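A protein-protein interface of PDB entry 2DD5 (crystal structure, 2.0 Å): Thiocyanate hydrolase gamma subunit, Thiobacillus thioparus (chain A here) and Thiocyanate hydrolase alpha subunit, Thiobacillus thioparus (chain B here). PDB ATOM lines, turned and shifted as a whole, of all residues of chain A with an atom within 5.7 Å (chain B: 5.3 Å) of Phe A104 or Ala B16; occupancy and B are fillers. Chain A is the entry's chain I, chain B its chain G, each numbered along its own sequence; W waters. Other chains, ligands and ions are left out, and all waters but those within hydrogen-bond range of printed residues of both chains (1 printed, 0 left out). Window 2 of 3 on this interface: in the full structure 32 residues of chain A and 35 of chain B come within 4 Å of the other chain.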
ATOM      1  N   TRP A  96      24.884 -18.824 -36.998  1.00  0.00           N
ATOM      2  CA  TRP A  96      24.810 -18.299 -35.641  1.00  0.00           C
ATOM      3  C   TRP A  96      25.283 -19.249 -34.553  1.00  0.00           C
ATOM      4  O   TRP A  96      25.682 -18.808 -33.475  1.00  0.00           O
ATOM      5  CB  TRP A  96      23.389 -17.806 -35.355  1.00  0.00           C
ATOM      6  CG  TRP A  96      23.116 -16.522 -36.075  1.00  0.00           C
ATOM      7  CD1 TRP A  96      23.124 -16.322 -37.428  1.00  0.00           C
ATOM      8  CD2 TRP A  96      22.901 -15.238 -35.482  1.00  0.00           C
ATOM      9  NE1 TRP A  96      22.937 -14.991 -37.713  1.00  0.00           N
ATOM     10  CE2 TRP A  96      22.797 -14.301 -36.537  1.00  0.00           C
ATOM     11  CE3 TRP A  96      22.787 -14.786 -34.160  1.00  0.00           C
ATOM     12  CZ2 TRP A  96      22.587 -12.936 -36.312  1.00  0.00           C
ATOM     13  CZ3 TRP A  96      22.575 -13.425 -33.936  1.00  0.00           C
ATOM     14  CH2 TRP A  96      22.479 -12.518 -35.008  1.00  0.00           C
ATOM     15  N   VAL A  97      25.261 -20.547 -34.832  1.00  0.00           N
ATOM     16  CA  VAL A  97      25.708 -21.515 -33.840  1.00  0.00           C
ATOM     17  C   VAL A  97      27.196 -21.848 -33.965  1.00  0.00           C
ATOM     18  O   VAL A  97      27.939 -21.786 -32.984  1.00  0.00           O
ATOM     19  CB  VAL A  97      24.909 -22.838 -33.944  1.00  0.00           C
ATOM     20  CG1 VAL A  97      25.410 -23.840 -32.899  1.00  0.00           C
ATOM     21  CG2 VAL A  97      23.430 -22.567 -33.753  1.00  0.00           C
ATOM     22  N   THR A  98      27.638 -22.159 -35.180  1.00  0.00           N
ATOM     23  CA  THR A  98      29.021 -22.569 -35.399  1.00  0.00           C
ATOM     24  C   THR A  98      30.057 -21.540 -35.848  1.00  0.00           C
ATOM     25  O   THR A  98      31.257 -21.825 -35.801  1.00  0.00           O
ATOM     26  CB  THR A  98      29.069 -23.761 -36.379  1.00  0.00           C
ATOM     27  OG1 THR A  98      28.552 -23.360 -37.652  1.00  0.00           O
ATOM     28  CG2 THR A  98      28.221 -24.910 -35.845  1.00  0.00           C
ATOM     29  N   PRO A 100      30.725 -18.513 -34.388  1.00  0.00           N
ATOM     30  CA  PRO A 100      31.463 -17.955 -33.244  1.00  0.00           C
ATOM     31  C   PRO A 100      32.401 -19.017 -32.651  1.00  0.00           C
ATOM     32  O   PRO A 100      32.138 -20.210 -32.770  1.00  0.00           O
ATOM     33  CB  PRO A 100      30.353 -17.564 -32.266  1.00  0.00           C
ATOM     34  CG  PRO A 100      29.163 -17.312 -33.172  1.00  0.00           C
ATOM     35  CD  PRO A 100      29.272 -18.457 -34.152  1.00  0.00           C
ATOM     36  N   THR A 102      32.850 -20.166 -29.717  1.00  0.00           N
ATOM     37  CA  THR A 102      32.223 -21.046 -28.733  1.00  0.00           C
ATOM     38  C   THR A 102      31.593 -22.293 -29.336  1.00  0.00           C
ATOM     39  O   THR A 102      31.506 -23.335 -28.688  1.00  0.00           O
ATOM     40  CB  THR A 102      31.080 -20.334 -28.006  1.00  0.00           C
ATOM     41  OG1 THR A 102      30.024 -20.093 -28.944  1.00  0.00           O
ATOM     42  CG2 THR A 102      31.542 -19.012 -27.421  1.00  0.00           C
ATOM     43  N   GLN A 103      31.124 -22.159 -30.569  1.00  0.00           N
ATOM     44  CA  GLN A 103      30.430 -23.224 -31.274  1.00  0.00           C
ATOM     45  C   GLN A 103      29.043 -23.454 -30.661  1.00  0.00           C
ATOM     46  O   GLN A 103      28.442 -24.520 -30.808  1.00  0.00           O
ATOM     47  CB  GLN A 103      31.235 -24.529 -31.286  1.00  0.00           C
ATOM     48  CG  GLN A 103      30.692 -25.517 -32.317  1.00  0.00           C
ATOM     49  CD  GLN A 103      31.451 -26.827 -32.363  1.00  0.00           C
ATOM     50  OE1 GLN A 103      30.946 -27.826 -32.877  1.00  0.00           O
ATOM     51  NE2 GLN A 103      32.666 -26.832 -31.830  1.00  0.00           N
ATOM     52  N   PHE A 104      28.547 -22.449 -29.940  1.00  0.00           N
ATOM     53  CA  PHE A 104      27.198 -22.503 -29.380  1.00  0.00           C
ATOM     54  C   PHE A 104      26.625 -21.088 -29.411  1.00  0.00           C
ATOM     55  O   PHE A 104      25.791 -20.713 -28.589  1.00  0.00           O
ATOM     56  CB  PHE A 104      27.161 -23.118 -27.958  1.00  0.00           C
ATOM     57  CG  PHE A 104      28.004 -22.408 -26.921  1.00  0.00           C
ATOM     58  CD1 PHE A 104      27.624 -21.172 -26.407  1.00  0.00           C
ATOM     59  CD2 PHE A 104      29.144 -23.020 -26.404  1.00  0.00           C
ATOM     60  CE1 PHE A 104      28.363 -20.559 -25.388  1.00  0.00           C
ATOM     61  CE2 PHE A 104      29.889 -22.413 -25.385  1.00  0.00           C
ATOM     62  CZ  PHE A 104      29.494 -21.180 -24.878  1.00  0.00           C
ATOM     63  N   GLY A 105      27.072 -20.327 -30.410  1.00  0.00           N
ATOM     64  CA  GLY A 105      26.638 -18.952 -30.581  1.00  0.00           C
ATOM     65  C   GLY A 105      27.408 -18.067 -29.624  1.00  0.00           C
ATOM     66  O   GLY A 105      27.989 -18.567 -28.661  1.00  0.00           O
ATOM     67  N   THR A 106      27.444 -16.764 -29.879  1.00  0.00           N
ATOM     68  CA  THR A 106      28.148 -15.878 -28.962  1.00  0.00           C
ATOM     69  C   THR A 106      27.348 -15.885 -27.667  1.00  0.00           C
ATOM     70  O   THR A 106      26.126 -16.073 -27.675  1.00  0.00           O
ATOM     71  CB  THR A 106      28.240 -14.430 -29.491  1.00  0.00           C
ATOM     72  OG1 THR A 106      26.924 -13.896 -29.666  1.00  0.00           O
ATOM     73  CG2 THR A 106      28.990 -14.394 -30.819  1.00  0.00           C
ATOM     74  N   PRO A 107      28.026 -15.715 -26.526  1.00  0.00           N
ATOM     75  CA  PRO A 107      27.306 -15.714 -25.249  1.00  0.00           C
ATOM     76  C   PRO A 107      26.260 -14.604 -25.134  1.00  0.00           C
ATOM     77  O   PRO A 107      25.193 -14.807 -24.554  1.00  0.00           O
ATOM     78  CB  PRO A 107      28.426 -15.546 -24.223  1.00  0.00           C
ATOM     79  CG  PRO A 107      29.611 -16.197 -24.902  1.00  0.00           C
ATOM     80  CD  PRO A 107      29.482 -15.666 -26.314  1.00  0.00           C
ATOM     81  N   CYS A 111      21.350 -17.339 -30.445  1.00  0.00           N
ATOM     82  CA  CYS A 111      21.140 -17.915 -31.771  1.00  0.00           C
ATOM     83  C   CYS A 111      19.708 -17.837 -32.300  1.00  0.00           C
ATOM     84  O   CYS A 111      19.164 -18.835 -32.775  1.00  0.00           O
ATOM     85  CB  CYS A 111      21.595 -19.378 -31.755  1.00  0.00           C
ATOM     86  SG  CYS A 111      23.221 -19.637 -30.987  1.00  0.00           S
ATOM     87  N   THR B  13      31.512 -25.805 -16.645  1.00  0.00           N
ATOM     88  CA  THR B  13      31.400 -26.537 -17.905  1.00  0.00           C
ATOM     89  C   THR B  13      29.975 -26.870 -18.340  1.00  0.00           C
ATOM     90  O   THR B  13      29.751 -27.262 -19.484  1.00  0.00           O
ATOM     91  CB  THR B  13      32.194 -27.862 -17.849  1.00  0.00           C
ATOM     92  OG1 THR B  13      31.596 -28.738 -16.887  1.00  0.00           O
ATOM     93  CG2 THR B  13      33.641 -27.601 -17.457  1.00  0.00           C
ATOM     94  N   HIS B  14      29.013 -26.704 -17.439  1.00  0.00           N
ATOM     95  CA  HIS B  14      27.623 -27.033 -17.737  1.00  0.00           C
ATOM     96  C   HIS B  14      27.007 -26.401 -18.984  1.00  0.00           C
ATOM     97  O   HIS B  14      26.409 -27.100 -19.800  1.00  0.00           O
ATOM     98  CB  HIS B  14      26.736 -26.725 -16.528  1.00  0.00           C
ATOM     99  CG  HIS B  14      25.272 -26.868 -16.806  1.00  0.00           C
ATOM    100  ND1 HIS B  14      24.511 -25.841 -17.323  1.00  0.00           N
ATOM    101  CD2 HIS B  14      24.445 -27.934 -16.702  1.00  0.00           C
ATOM    102  CE1 HIS B  14      23.277 -26.269 -17.525  1.00  0.00           C
ATOM    103  NE2 HIS B  14      23.212 -27.536 -17.157  1.00  0.00           N
ATOM    104  N   HIS B  15      27.138 -25.087 -19.139  1.00  0.00           N
ATOM    105  CA  HIS B  15      26.549 -24.421 -20.296  1.00  0.00           C
ATOM    106  C   HIS B  15      27.124 -24.923 -21.619  1.00  0.00           C
ATOM    107  O   HIS B  15      26.380 -25.250 -22.543  1.00  0.00           O
ATOM    108  CB  HIS B  15      26.738 -22.904 -20.198  1.00  0.00           C
ATOM    109  CG  HIS B  15      26.024 -22.141 -21.272  1.00  0.00           C
ATOM    110  ND1 HIS B  15      24.649 -22.086 -21.355  1.00  0.00           N
ATOM    111  CD2 HIS B  15      26.494 -21.430 -22.324  1.00  0.00           C
ATOM    112  CE1 HIS B  15      24.302 -21.373 -22.413  1.00  0.00           C
ATOM    113  NE2 HIS B  15      25.403 -20.964 -23.018  1.00  0.00           N
ATOM    114  N   ALA B  16      28.448 -24.981 -21.705  1.00  0.00           N
ATOM    115  CA  ALA B  16      29.118 -25.436 -22.918  1.00  0.00           C
ATOM    116  C   ALA B  16      28.737 -26.869 -23.291  1.00  0.00           C
ATOM    117  O   ALA B  16      28.429 -27.157 -24.449  1.00  0.00           O
ATOM    118  CB  ALA B  16      30.631 -25.328 -22.746  1.00  0.00           C
ATOM    119  N   LYS B  17      28.759 -27.767 -22.314  1.00  0.00           N
ATOM    120  CA  LYS B  17      28.418 -29.160 -22.573  1.00  0.00           C
ATOM    121  C   LYS B  17      26.981 -29.307 -23.056  1.00  0.00           C
ATOM    122  O   LYS B  17      26.659 -30.215 -23.821  1.00  0.00           O
ATOM    123  CB  LYS B  17      28.639 -30.004 -21.314  1.00  0.00           C
ATOM    124  CG  LYS B  17      30.108 -30.161 -20.942  1.00  0.00           C
ATOM    125  CD  LYS B  17      30.295 -31.000 -19.684  1.00  0.00           C
ATOM    126  CE  LYS B  17      31.777 -31.144 -19.345  1.00  0.00           C
ATOM    127  NZ  LYS B  17      32.010 -31.881 -18.068  1.00  0.00           N
ATOM    128  N   MET B  18      26.120 -28.398 -22.618  1.00  0.00           N
ATOM    129  CA  MET B  18      24.716 -28.434 -22.997  1.00  0.00           C
ATOM    130  C   MET B  18      24.401 -27.774 -24.342  1.00  0.00           C
ATOM    131  O   MET B  18      23.569 -28.271 -25.101  1.00  0.00           O
ATOM    132  CB  MET B  18      23.880 -27.768 -21.900  1.00  0.00           C
ATOM    133  CG  MET B  18      22.461 -27.417 -22.312  1.00  0.00           C
ATOM    134  SD  MET B  18      21.563 -26.552 -21.002  1.00  0.00           S
ATOM    135  CE  MET B  18      20.407 -27.817 -20.488  1.00  0.00           C
ATOM    136  N   ALA B  19      25.072 -26.667 -24.641  1.00  0.00           N
ATOM    137  CA  ALA B  19      24.798 -25.921 -25.868  1.00  0.00           C
ATOM    138  C   ALA B  19      25.731 -26.091 -27.065  1.00  0.00           C
ATOM    139  O   ALA B  19      25.361 -25.718 -28.181  1.00  0.00           O
ATOM    140  CB  ALA B  19      24.682 -24.437 -25.530  1.00  0.00           C
ATOM    141  N   THR B  20      26.926 -26.636 -26.858  1.00  0.00           N
ATOM    142  CA  THR B  20      27.863 -26.795 -27.970  1.00  0.00           C
ATOM    143  C   THR B  20      27.244 -27.571 -29.133  1.00  0.00           C
ATOM    144  O   THR B  20      26.665 -28.637 -28.941  1.00  0.00           O
ATOM    145  CB  THR B  20      29.167 -27.494 -27.520  1.00  0.00           C
ATOM    146  OG1 THR B  20      29.843 -26.674 -26.555  1.00  0.00           O
ATOM    147  CG2 THR B  20      30.092 -27.715 -28.706  1.00  0.00           C
ATOM    148  N   GLY B  21      27.353 -27.010 -30.335  1.00  0.00           N
ATOM    149  CA  GLY B  21      26.807 -27.650 -31.521  1.00  0.00           C
ATOM    150  C   GLY B  21      25.295 -27.554 -31.629  1.00  0.00           C
ATOM    151  O   GLY B  21      24.702 -28.050 -32.590  1.00  0.00           O
ATOM    152  N   ILE B  22      24.672 -26.909 -30.647  1.00  0.00           N
ATOM    153  CA  ILE B  22      23.223 -26.759 -30.619  1.00  0.00           C
ATOM    154  C   ILE B  22      22.809 -25.290 -30.595  1.00  0.00           C
ATOM    155  O   ILE B  22      21.962 -24.858 -31.378  1.00  0.00           O
ATOM    156  CB  ILE B  22      22.623 -27.442 -29.376  1.00  0.00           C
ATOM    157  CG1 ILE B  22      23.011 -28.922 -29.355  1.00  0.00           C
ATOM    158  CG2 ILE B  22      21.112 -27.276 -29.369  1.00  0.00           C
ATOM    159  CD1 ILE B  22      22.563 -29.688 -30.579  1.00  0.00           C
ATOM    160  N   GLY B  23      23.403 -24.529 -29.681  1.00  0.00           N
ATOM    161  CA  GLY B  23      23.075 -23.120 -29.572  1.00  0.00           C
ATOM    162  C   GLY B  23      22.105 -22.816 -28.445  1.00  0.00           C
ATOM    163  O   GLY B  23      21.473 -23.714 -27.889  1.00  0.00           O
ATOM    164  N   ASP B  24      22.001 -21.532 -28.116  1.00  0.00           N
ATOM    165  CA  ASP B  24      21.121 -21.027 -27.061  1.00  0.00           C
ATOM    166  C   ASP B  24      20.211 -20.040 -27.794  1.00  0.00           C
ATOM    167  O   ASP B  24      20.706 -19.157 -28.486  1.00  0.00           O
ATOM    168  CB  ASP B  24      21.976 -20.298 -26.013  1.00  0.00           C
ATOM    169  CG  ASP B  24      21.167 -19.767 -24.839  1.00  0.00           C
ATOM    170  OD1 ASP B  24      19.920 -19.788 -24.892  1.00  0.00           O
ATOM    171  OD2 ASP B  24      21.798 -19.315 -23.858  1.00  0.00           O
HETATM  172  O   HOH W   1      32.067 -25.058 -26.769  1.00  0.00           O
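N of Cys A111 is in hydrogen-bond range of O of Asp B24 (2.7 Å). The backbone carbonyl oxygen (O) of Gln A103 lies within hydrogen-bond range of the backbone NH (N) of Gly B21 (2.8 Å).
CG1 of Val A97 touches C of Gly B21, at 3.9 Å. Val A97 touches Ile B22 (CG2 to O, 3.6 Å). Gly B23 touches Val A97 (N to CG1, 3.9 Å). Gln A103 touches Thr B20. CD2 of His B15 touches CE1 of Phe A104, 3.7 Å away. Phe A104 touches Ala B16. Ala B19 touches Phe A104. Thr B20 touches Phe A104 (N to CB, 3.7 Å). Asp B24 touches Phe A104 (N to O, 3.9 Å). Gly B23 touches Cys A111 (CA to SG, 3.8 Å).
Hydrophobic or aromatic side chains of chain A within 4 Å of the printed part of chain B: Val A97 and Phe A104. Of the 12 printed residues of chain B, 8 touch a printed residue of chain A. Printed residues of chain B that touch a printed residue of chain A: His B15, Ala B16, Ala B19, Thr B20, Gly B21, Ile B22, Gly B23 and Asp B24. Among the printed residues, 13 pairs touch across the chains.
Of chain A, only Phe A104 (3.98 Å) comes within 4 Å of Ala B16. Printed residues of chain A within 4 Å of Gly B23: Val A97, Phe A104 and Cys A111. Printed residues of chain B within 4 Å of Gln A103: Thr B20 (3.7 Å) and Gly B21 (2.8 Å). Printed residues of chain A within 4 Å of Thr B20: Gln A103 (3.7 Å) and Phe A104 (3.7 Å). Printed residues of chain B within 4 Å of Cys A111: Gly B23 (3.8 Å) and Asp B24 (2.7 Å). Of the printed residues of chain A, Ile B22 touches Val A97 (3.6 Å). The nearest residue of chain B that does not touch Phe A104 is Gly B21 (4.6 Å).
N of Phe A104 is in hydrogen-bond range of OG1 of Thr A102, 3.0 Å away. The side-chain sulfur of Cys A111 lies within hydrogen-bond range of the backbone carbonyl oxygen of Phe A104, 3.7 Å away. O of Ala B16 is in hydrogen-bond range of OG1 of Thr B20 (2.6 Å). O of Val A97 is in hydrogen-bond range of N of Gly A105, 3.1 Å away. O of Val A97 is in hydrogen-bond range of N of Phe A104. The backbone carbonyl oxygen of Trp A96 sits at hydrogen-bond distance from the side-chain sulfur of Cys A111, at 3.6 Å.
Water W1 lies within hydrogen-bond range of the backbone carbonyl oxygen of Thr A102 (2.6 Å) and the side-chain hydroxyl of Thr B20 (2.8 Å).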
